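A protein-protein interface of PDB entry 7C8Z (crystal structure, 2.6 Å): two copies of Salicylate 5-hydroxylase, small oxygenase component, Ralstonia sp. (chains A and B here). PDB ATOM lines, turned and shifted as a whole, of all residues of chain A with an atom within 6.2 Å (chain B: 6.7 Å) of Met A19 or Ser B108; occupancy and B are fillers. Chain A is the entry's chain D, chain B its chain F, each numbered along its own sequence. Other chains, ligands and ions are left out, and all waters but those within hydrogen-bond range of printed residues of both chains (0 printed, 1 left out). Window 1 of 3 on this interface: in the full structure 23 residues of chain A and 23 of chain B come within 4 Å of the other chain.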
ATOM      1  N   TYR A  14      14.644 -23.402   8.212  1.00  0.00           N
ATOM      2  CA  TYR A  14      15.982 -23.705   7.698  1.00  0.00           C
ATOM      3  C   TYR A  14      17.004 -23.718   8.829  1.00  0.00           C
ATOM      4  O   TYR A  14      17.797 -24.667   8.971  1.00  0.00           O
ATOM      5  CB  TYR A  14      16.382 -22.696   6.616  1.00  0.00           C
ATOM      6  CG  TYR A  14      15.878 -23.075   5.250  1.00  0.00           C
ATOM      7  CD1 TYR A  14      16.588 -23.964   4.451  1.00  0.00           C
ATOM      8  CD2 TYR A  14      14.680 -22.571   4.766  1.00  0.00           C
ATOM      9  CE1 TYR A  14      16.119 -24.332   3.196  1.00  0.00           C
ATOM     10  CE2 TYR A  14      14.203 -22.936   3.518  1.00  0.00           C
ATOM     11  CZ  TYR A  14      14.929 -23.817   2.739  1.00  0.00           C
ATOM     12  OH  TYR A  14      14.460 -24.185   1.499  1.00  0.00           O
ATOM     13  N   SER A  15      16.961 -22.688   9.680  1.00  0.00           N
ATOM     14  CA  SER A  15      17.919 -22.584  10.774  1.00  0.00           C
ATOM     15  C   SER A  15      17.715 -23.688  11.808  1.00  0.00           C
ATOM     16  O   SER A  15      18.691 -24.268  12.297  1.00  0.00           O
ATOM     17  CB  SER A  15      17.806 -21.207  11.425  1.00  0.00           C
ATOM     18  OG  SER A  15      18.941 -20.916  12.229  1.00  0.00           O
ATOM     19  N   ASP A  16      16.459 -23.986  12.156  1.00  0.00           N
ATOM     20  CA  ASP A  16      16.162 -25.043  13.116  1.00  0.00           C
ATOM     21  C   ASP A  16      16.708 -26.372  12.637  1.00  0.00           C
ATOM     22  O   ASP A  16      17.357 -27.094  13.398  1.00  0.00           O
ATOM     23  CB  ASP A  16      14.653 -25.155  13.340  1.00  0.00           C
ATOM     24  CG  ASP A  16      14.118 -24.122  14.302  1.00  0.00           C
ATOM     25  OD1 ASP A  16      14.916 -23.555  15.075  1.00  0.00           O
ATOM     26  OD2 ASP A  16      12.887 -23.880  14.285  1.00  0.00           O
ATOM     27  N   TYR A  17      16.429 -26.724  11.379  1.00  0.00           N
ATOM     28  CA  TYR A  17      16.953 -27.963  10.819  1.00  0.00           C
ATOM     29  C   TYR A  17      18.465 -28.016  10.963  1.00  0.00           C
ATOM     30  O   TYR A  17      19.021 -28.964  11.538  1.00  0.00           O
ATOM     31  CB  TYR A  17      16.540 -28.069   9.351  1.00  0.00           C
ATOM     32  CG  TYR A  17      16.919 -29.358   8.653  1.00  0.00           C
ATOM     33  CD1 TYR A  17      18.221 -29.587   8.224  1.00  0.00           C
ATOM     34  CD2 TYR A  17      15.965 -30.329   8.389  1.00  0.00           C
ATOM     35  CE1 TYR A  17      18.563 -30.756   7.572  1.00  0.00           C
ATOM     36  CE2 TYR A  17      16.298 -31.501   7.738  1.00  0.00           C
ATOM     37  CZ  TYR A  17      17.595 -31.708   7.330  1.00  0.00           C
ATOM     38  OH  TYR A  17      17.927 -32.875   6.678  1.00  0.00           O
ATOM     39  N   ALA A  18      19.144 -26.968  10.485  1.00  0.00           N
ATOM     40  CA  ALA A  18      20.600 -26.950  10.525  1.00  0.00           C
ATOM     41  C   ALA A  18      21.119 -27.139  11.948  1.00  0.00           C
ATOM     42  O   ALA A  18      21.933 -28.029  12.210  1.00  0.00           O
ATOM     43  CB  ALA A  18      21.115 -25.642   9.924  1.00  0.00           C
ATOM     44  N   MET A  19      20.639 -26.328  12.889  1.00  0.00           N
ATOM     45  CA  MET A  19      21.227 -26.323  14.225  1.00  0.00           C
ATOM     46  C   MET A  19      20.824 -27.544  15.040  1.00  0.00           C
ATOM     47  O   MET A  19      21.606 -28.003  15.881  1.00  0.00           O
ATOM     48  CB  MET A  19      20.833 -25.047  14.977  1.00  0.00           C
ATOM     49  CG  MET A  19      21.173 -23.761  14.229  1.00  0.00           C
ATOM     50  SD  MET A  19      21.537 -22.336  15.275  1.00  0.00           S
ATOM     51  CE  MET A  19      22.863 -22.974  16.274  1.00  0.00           C
ATOM     52  N   VAL A  20      19.624 -28.083  14.809  1.00  0.00           N
ATOM     53  CA  VAL A  20      19.186 -29.271  15.523  1.00  0.00           C
ATOM     54  C   VAL A  20      19.957 -30.498  15.049  1.00  0.00           C
ATOM     55  O   VAL A  20      20.346 -31.347  15.865  1.00  0.00           O
ATOM     56  CB  VAL A  20      17.658 -29.434  15.382  1.00  0.00           C
ATOM     57  CG1 VAL A  20      17.225 -30.840  15.704  1.00  0.00           C
ATOM     58  CG2 VAL A  20      16.938 -28.452  16.298  1.00  0.00           C
ATOM     59  N   CYS A  21      20.241 -30.597  13.736  1.00  0.00           N
ATOM     60  CA  CYS A  21      21.017 -31.756  13.290  1.00  0.00           C
ATOM     61  C   CYS A  21      22.499 -31.618  13.569  1.00  0.00           C
ATOM     62  O   CYS A  21      23.244 -32.580  13.352  1.00  0.00           O
ATOM     63  CB  CYS A  21      20.862 -32.023  11.785  1.00  0.00           C
ATOM     64  SG  CYS A  21      19.223 -32.104  11.083  1.00  0.00           S
ATOM     65  N   ASP A  22      22.929 -30.500  14.133  1.00  0.00           N
ATOM     66  CA  ASP A  22      24.290 -30.379  14.615  1.00  0.00           C
ATOM     67  C   ASP A  22      24.416 -30.656  16.104  1.00  0.00           C
ATOM     68  O   ASP A  22      25.539 -30.806  16.598  1.00  0.00           O
ATOM     69  CB  ASP A  22      24.821 -28.978  14.306  1.00  0.00           C
ATOM     70  CG  ASP A  22      24.892 -28.694  12.822  1.00  0.00           C
ATOM     71  OD1 ASP A  22      24.823 -29.653  12.016  1.00  0.00           O
ATOM     72  OD2 ASP A  22      25.024 -27.508  12.461  1.00  0.00           O
ATOM     73  N   SER A  23      23.298 -30.768  16.813  1.00  0.00           N
ATOM     74  CA  SER A  23      23.287 -30.841  18.262  1.00  0.00           C
ATOM     75  C   SER A  23      23.121 -32.284  18.721  1.00  0.00           C
ATOM     76  O   SER A  23      22.929 -33.203  17.922  1.00  0.00           O
ATOM     77  CB  SER A  23      22.166 -29.966  18.819  1.00  0.00           C
ATOM     78  OG  SER A  23      20.913 -30.453  18.373  1.00  0.00           O
ATOM     79  N   ARG A  83      28.653 -28.953  11.469  1.00  0.00           N
ATOM     80  CA  ARG A  83      28.146 -27.593  11.604  1.00  0.00           C
ATOM     81  C   ARG A  83      27.581 -27.157  10.259  1.00  0.00           C
ATOM     82  O   ARG A  83      28.337 -26.980   9.301  1.00  0.00           O
ATOM     83  CB  ARG A  83      29.254 -26.654  12.078  1.00  0.00           C
ATOM     84  CG  ARG A  83      28.832 -25.219  12.241  1.00  0.00           C
ATOM     85  CD  ARG A  83      27.798 -25.077  13.316  1.00  0.00           C
ATOM     86  NE  ARG A  83      28.083 -25.932  14.455  1.00  0.00           N
ATOM     87  CZ  ARG A  83      27.177 -26.271  15.367  1.00  0.00           C
ATOM     88  NH1 ARG A  83      25.935 -25.817  15.260  1.00  0.00           N
ATOM     89  NH2 ARG A  83      27.514 -27.065  16.375  1.00  0.00           N
ATOM     90  N   HIS A  84      26.259 -27.027  10.171  1.00  0.00           N
ATOM     91  CA  HIS A  84      25.621 -26.573   8.942  1.00  0.00           C
ATOM     92  C   HIS A  84      25.671 -25.052   8.873  1.00  0.00           C
ATOM     93  O   HIS A  84      25.131 -24.371   9.750  1.00  0.00           O
ATOM     94  CB  HIS A  84      24.167 -27.030   8.869  1.00  0.00           C
ATOM     95  CG  HIS A  84      23.989 -28.498   8.648  1.00  0.00           C
ATOM     96  ND1 HIS A  84      24.462 -29.448   9.528  1.00  0.00           N
ATOM     97  CD2 HIS A  84      23.351 -29.179   7.667  1.00  0.00           C
ATOM     98  CE1 HIS A  84      24.144 -30.652   9.085  1.00  0.00           C
ATOM     99  NE2 HIS A  84      23.468 -30.518   7.958  1.00  0.00           N
ATOM    100  N   ILE A  85      26.276 -24.525   7.814  1.00  0.00           N
ATOM    101  CA  ILE A  85      26.201 -23.111   7.468  1.00  0.00           C
ATOM    102  C   ILE A  85      25.266 -23.024   6.268  1.00  0.00           C
ATOM    103  O   ILE A  85      25.635 -23.398   5.150  1.00  0.00           O
ATOM    104  CB  ILE A  85      27.575 -22.513   7.151  1.00  0.00           C
ATOM    105  CG1 ILE A  85      28.579 -22.862   8.252  1.00  0.00           C
ATOM    106  CG2 ILE A  85      27.461 -21.019   6.975  1.00  0.00           C
ATOM    107  CD1 ILE A  85      28.187 -22.366   9.618  1.00  0.00           C
ATOM    108  N   ILE B  85      31.123 -16.195   8.205  1.00  0.00           N
ATOM    109  CA  ILE B  85      29.956 -16.649   7.469  1.00  0.00           C
ATOM    110  C   ILE B  85      28.944 -17.102   8.511  1.00  0.00           C
ATOM    111  O   ILE B  85      29.062 -18.195   9.075  1.00  0.00           O
ATOM    112  CB  ILE B  85      30.299 -17.773   6.484  1.00  0.00           C
ATOM    113  CG1 ILE B  85      31.436 -17.346   5.553  1.00  0.00           C
ATOM    114  CG2 ILE B  85      29.083 -18.145   5.662  1.00  0.00           C
ATOM    115  CD1 ILE B  85      31.087 -16.152   4.674  1.00  0.00           C
ATOM    116  N   VAL B  86      27.952 -16.262   8.780  1.00  0.00           N
ATOM    117  CA  VAL B  86      26.932 -16.547   9.779  1.00  0.00           C
ATOM    118  C   VAL B  86      25.706 -17.091   9.061  1.00  0.00           C
ATOM    119  O   VAL B  86      25.084 -16.388   8.255  1.00  0.00           O
ATOM    120  CB  VAL B  86      26.582 -15.298  10.600  1.00  0.00           C
ATOM    121  CG1 VAL B  86      25.626 -15.668  11.716  1.00  0.00           C
ATOM    122  CG2 VAL B  86      27.847 -14.653  11.160  1.00  0.00           C
ATOM    123  N   GLY B  87      25.348 -18.333   9.365  1.00  0.00           N
ATOM    124  CA  GLY B  87      24.165 -18.938   8.796  1.00  0.00           C
ATOM    125  C   GLY B  87      22.899 -18.237   9.250  1.00  0.00           C
ATOM    126  O   GLY B  87      22.905 -17.329  10.082  1.00  0.00           O
ATOM    127  N   THR B  88      21.785 -18.685   8.688  1.00  0.00           N
ATOM    128  CA  THR B  88      20.486 -18.093   8.988  1.00  0.00           C
ATOM    129  C   THR B  88      20.213 -18.144  10.487  1.00  0.00           C
ATOM    130  O   THR B  88      20.209 -19.237  11.071  1.00  0.00           O
ATOM    131  CB  THR B  88      19.376 -18.820   8.228  1.00  0.00           C
ATOM    132  OG1 THR B  88      19.548 -18.623   6.816  1.00  0.00           O
ATOM    133  CG2 THR B  88      18.009 -18.294   8.654  1.00  0.00           C
ATOM    134  N   PRO B  89      20.038 -17.005  11.150  1.00  0.00           N
ATOM    135  CA  PRO B  89      19.738 -17.025  12.586  1.00  0.00           C
ATOM    136  C   PRO B  89      18.343 -17.569  12.856  1.00  0.00           C
ATOM    137  O   PRO B  89      17.469 -17.588  11.986  1.00  0.00           O
ATOM    138  CB  PRO B  89      19.852 -15.551  12.998  1.00  0.00           C
ATOM    139  CG  PRO B  89      20.646 -14.902  11.917  1.00  0.00           C
ATOM    140  CD  PRO B  89      20.267 -15.640  10.657  1.00  0.00           C
ATOM    141  N   ARG B  90      18.149 -18.041  14.088  1.00  0.00           N
ATOM    142  CA  ARG B  90      16.856 -18.530  14.543  1.00  0.00           C
ATOM    143  C   ARG B  90      16.478 -17.822  15.836  1.00  0.00           C
ATOM    144  O   ARG B  90      17.321 -17.624  16.722  1.00  0.00           O
ATOM    145  CB  ARG B  90      16.867 -20.068  14.734  1.00  0.00           C
ATOM    146  CG  ARG B  90      17.560 -20.573  16.007  1.00  0.00           C
ATOM    147  CD  ARG B  90      18.167 -21.977  15.850  1.00  0.00           C
ATOM    148  NE  ARG B  90      17.197 -23.035  16.116  1.00  0.00           N
ATOM    149  CZ  ARG B  90      17.277 -23.920  17.108  1.00  0.00           C
ATOM    150  NH1 ARG B  90      18.289 -23.903  17.959  1.00  0.00           N
ATOM    151  NH2 ARG B  90      16.327 -24.833  17.245  1.00  0.00           N
ATOM    152  N   GLU B 106      19.866 -17.783  18.214  1.00  0.00           N
ATOM    153  CA  GLU B 106      21.065 -18.546  17.907  1.00  0.00           C
ATOM    154  C   GLU B 106      21.409 -18.378  16.436  1.00  0.00           C
ATOM    155  O   GLU B 106      20.567 -18.001  15.621  1.00  0.00           O
ATOM    156  CB  GLU B 106      20.894 -20.040  18.230  1.00  0.00           C
ATOM    157  CG  GLU B 106      21.011 -20.390  19.697  1.00  0.00           C
ATOM    158  CD  GLU B 106      20.736 -21.864  19.967  1.00  0.00           C
ATOM    159  OE1 GLU B 106      20.632 -22.636  18.989  1.00  0.00           O
ATOM    160  OE2 GLU B 106      20.623 -22.247  21.158  1.00  0.00           O
ATOM    161  N   ALA B 107      22.666 -18.659  16.106  1.00  0.00           N
ATOM    162  CA  ALA B 107      23.085 -18.715  14.714  1.00  0.00           C
ATOM    163  C   ALA B 107      24.398 -19.473  14.637  1.00  0.00           C
ATOM    164  O   ALA B 107      25.291 -19.253  15.463  1.00  0.00           O
ATOM    165  CB  ALA B 107      23.239 -17.316  14.120  1.00  0.00           C
ATOM    166  N   SER B 108      24.494 -20.392  13.681  1.00  0.00           N
ATOM    167  CA  SER B 108      25.763 -21.046  13.417  1.00  0.00           C
ATOM    168  C   SER B 108      26.677 -20.087  12.672  1.00  0.00           C
ATOM    169  O   SER B 108      26.222 -19.214  11.928  1.00  0.00           O
ATOM    170  CB  SER B 108      25.556 -22.319  12.603  1.00  0.00           C
ATOM    171  OG  SER B 108      25.172 -23.389  13.446  1.00  0.00           O
ATOM    172  N   TYR B 109      27.978 -20.267  12.863  1.00  0.00           N
ATOM    173  CA  TYR B 109      28.967 -19.410  12.233  1.00  0.00           C
ATOM    174  C   TYR B 109      30.148 -20.254  11.788  1.00  0.00           C
ATOM    175  O   TYR B 109      30.436 -21.306  12.364  1.00  0.00           O
ATOM    176  CB  TYR B 109      29.447 -18.295  13.181  1.00  0.00           C
ATOM    177  CG  TYR B 109      30.305 -18.785  14.334  1.00  0.00           C
ATOM    178  CD1 TYR B 109      31.674 -18.981  14.180  1.00  0.00           C
ATOM    179  CD2 TYR B 109      29.746 -19.045  15.576  1.00  0.00           C
ATOM    180  CE1 TYR B 109      32.453 -19.432  15.224  1.00  0.00           C
ATOM    181  CE2 TYR B 109      30.520 -19.489  16.629  1.00  0.00           C
ATOM    182  CZ  TYR B 109      31.870 -19.680  16.448  1.00  0.00           C
ATOM    183  OH  TYR B 109      32.639 -20.123  17.497  1.00  0.00           O
ATOM    184  N   ALA B 110      30.829 -19.771  10.753  1.00  0.00           N
ATOM    185  CA  ALA B 110      32.113 -20.308  10.323  1.00  0.00           C
ATOM    186  C   ALA B 110      33.060 -19.138  10.118  1.00  0.00           C
ATOM    187  O   ALA B 110      32.788 -18.257   9.298  1.00  0.00           O
ATOM    188  CB  ALA B 110      31.970 -21.120   9.036  1.00  0.00           C
ATOM    189  N   GLY B 126      31.377 -22.934  14.934  1.00  0.00           N
ATOM    190  CA  GLY B 126      30.557 -23.208  16.094  1.00  0.00           C
ATOM    191  C   GLY B 126      29.216 -22.522  15.961  1.00  0.00           C
ATOM    192  O   GLY B 126      28.695 -22.404  14.848  1.00  0.00           O
ATOM    193  N   TYR B 127      28.638 -22.066  17.070  1.00  0.00           N
ATOM    194  CA  TYR B 127      27.400 -21.312  16.967  1.00  0.00           C
ATOM    195  C   TYR B 127      27.331 -20.252  18.052  1.00  0.00           C
ATOM    196  O   TYR B 127      27.937 -20.387  19.121  1.00  0.00           O
ATOM    197  CB  TYR B 127      26.170 -22.227  17.039  1.00  0.00           C
ATOM    198  CG  TYR B 127      25.963 -22.956  18.348  1.00  0.00           C
ATOM    199  CD1 TYR B 127      26.669 -24.116  18.640  1.00  0.00           C
ATOM    200  CD2 TYR B 127      25.031 -22.510  19.274  1.00  0.00           C
ATOM    201  CE1 TYR B 127      26.472 -24.793  19.824  1.00  0.00           C
ATOM    202  CE2 TYR B 127      24.823 -23.186  20.464  1.00  0.00           C
ATOM    203  CZ  TYR B 127      25.550 -24.325  20.732  1.00  0.00           C
ATOM    204  OH  TYR B 127      25.350 -25.006  21.911  1.00  0.00           O
ATOM    205  N   TYR B 128      26.563 -19.204  17.766  1.00  0.00           N
ATOM    206  CA  TYR B 128      26.271 -18.164  18.738  1.00  0.00           C
ATOM    207  C   TYR B 128      25.018 -18.536  19.521  1.00  0.00           C
ATOM    208  O   TYR B 128      24.076 -19.113  18.972  1.00  0.00           O
ATOM    209  CB  TYR B 128      26.052 -16.815  18.052  1.00  0.00           C
ATOM    210  CG  TYR B 128      27.252 -16.277  17.322  1.00  0.00           C
ATOM    211  CD1 TYR B 128      28.407 -15.936  18.011  1.00  0.00           C
ATOM    212  CD2 TYR B 128      27.231 -16.097  15.942  1.00  0.00           C
ATOM    213  CE1 TYR B 128      29.512 -15.438  17.352  1.00  0.00           C
ATOM    214  CE2 TYR B 128      28.336 -15.594  15.270  1.00  0.00           C
ATOM    215  CZ  TYR B 128      29.475 -15.267  15.984  1.00  0.00           C
ATOM    216  OH  TYR B 128      30.588 -14.770  15.341  1.00  0.00           O
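OG of Ser A15 is in hydrogen-bond range of O of Thr B88 (2.4 Å). The side-chain carboxylate (OD1) of Asp A16 lies within salt-bridge range of the guanidinium group (NE) of Arg B90, 2.6 Å away. The guanidinium group (NH1) of Arg A83 lies close to the side-chain hydroxyl (OG) of Ser B108.
The side-chain hydroxyl (OG) of Ser A23 lies within hydrogen-bond range of the backbone carbonyl oxygen (O) of Val A20. The backbone NH (N) of Ile B85 is in hydrogen-bond range of the backbone carbonyl oxygen (O) of Ala B110. The backbone NH (N) of Gly B87 sits at hydrogen-bond distance from the backbone carbonyl oxygen (O) of Ser B108 (2.8 Å). The guanidinium group (NH1) of Arg B90 is in salt-bridge range of the side-chain carboxylate (OE1) of Glu B106, 2.9 Å away. The backbone carbonyl oxygen of Ala B107 is in hydrogen-bond range of the backbone NH of Tyr B128, 2.6 Å away. The backbone NH of Tyr B109 lies within hydrogen-bond range of the backbone carbonyl oxygen of Gly B126, at 3.0 Å.
Ser A15 touches Arg B90 (OG to CB, 3.4 Å). Met A19 touches Arg B90. SD of Met A19 touches N of Ala B107, at 3.9 Å. Met A19 touches Ser B108. Tyr B127 touches Met A19 (CB to CE, 3.5 Å). Arg B90 touches Val A20 (NH2 to CG2, 3.8 Å). CG2 of Ile A85 touches CG2 of Ile B85 (3.6 Å). Ser B108 touches Ile A85 (CB to CD1, 3.98 Å). Tyr B109 touches Ile A85. Ile A85 touches Ala B110.
Of chain B, only Arg B90, Glu B106, Ala B107, Ser B108 and Tyr B127 come within 4 Å of Met A19. Of chain A, only Met A19, Arg A83, His A84 and Ile A85 come within 4 Å of Ser B108. Printed residues of chain A within 4 Å of Glu B106: Met A19 (3.5 Å). Of the printed residues of chain A, Tyr B127 touches Met A19 (3.5 Å) and Arg A83 (3.8 Å). The nearest residue of chain B that does not touch Met A19 is Tyr B128 (4.9 Å). The nearest printed residue of chain A that does not touch Tyr B127 is Ser A23 (6.7 Å).
Of the 13 printed residues of chain A, 7 touch a printed residue of chain B. Hydrophobic or aromatic side chains of chain A that line the printed part of chain B: Met A19, Val A20 and Ile A85. Hydrophobic or aromatic side chains of chain B that line the printed part of chain A: Ile B85, Ala B110 and Tyr B127. Among the printed residues, 18 pairs touch across the chains. Among the printed residues, Asp or Glu carboxylates within 4 Å of a Lys or Arg side-chain nitrogen of the other chain: Asp A16 with Arg B90 (2.6 Å).
Ile B85 touches its own counterpart, Ile A85. Position printed for both chains: 85. Of the 18 pairs that touch across the chains among the printed residues, 1 has its exchanged pair printed and touching as well.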
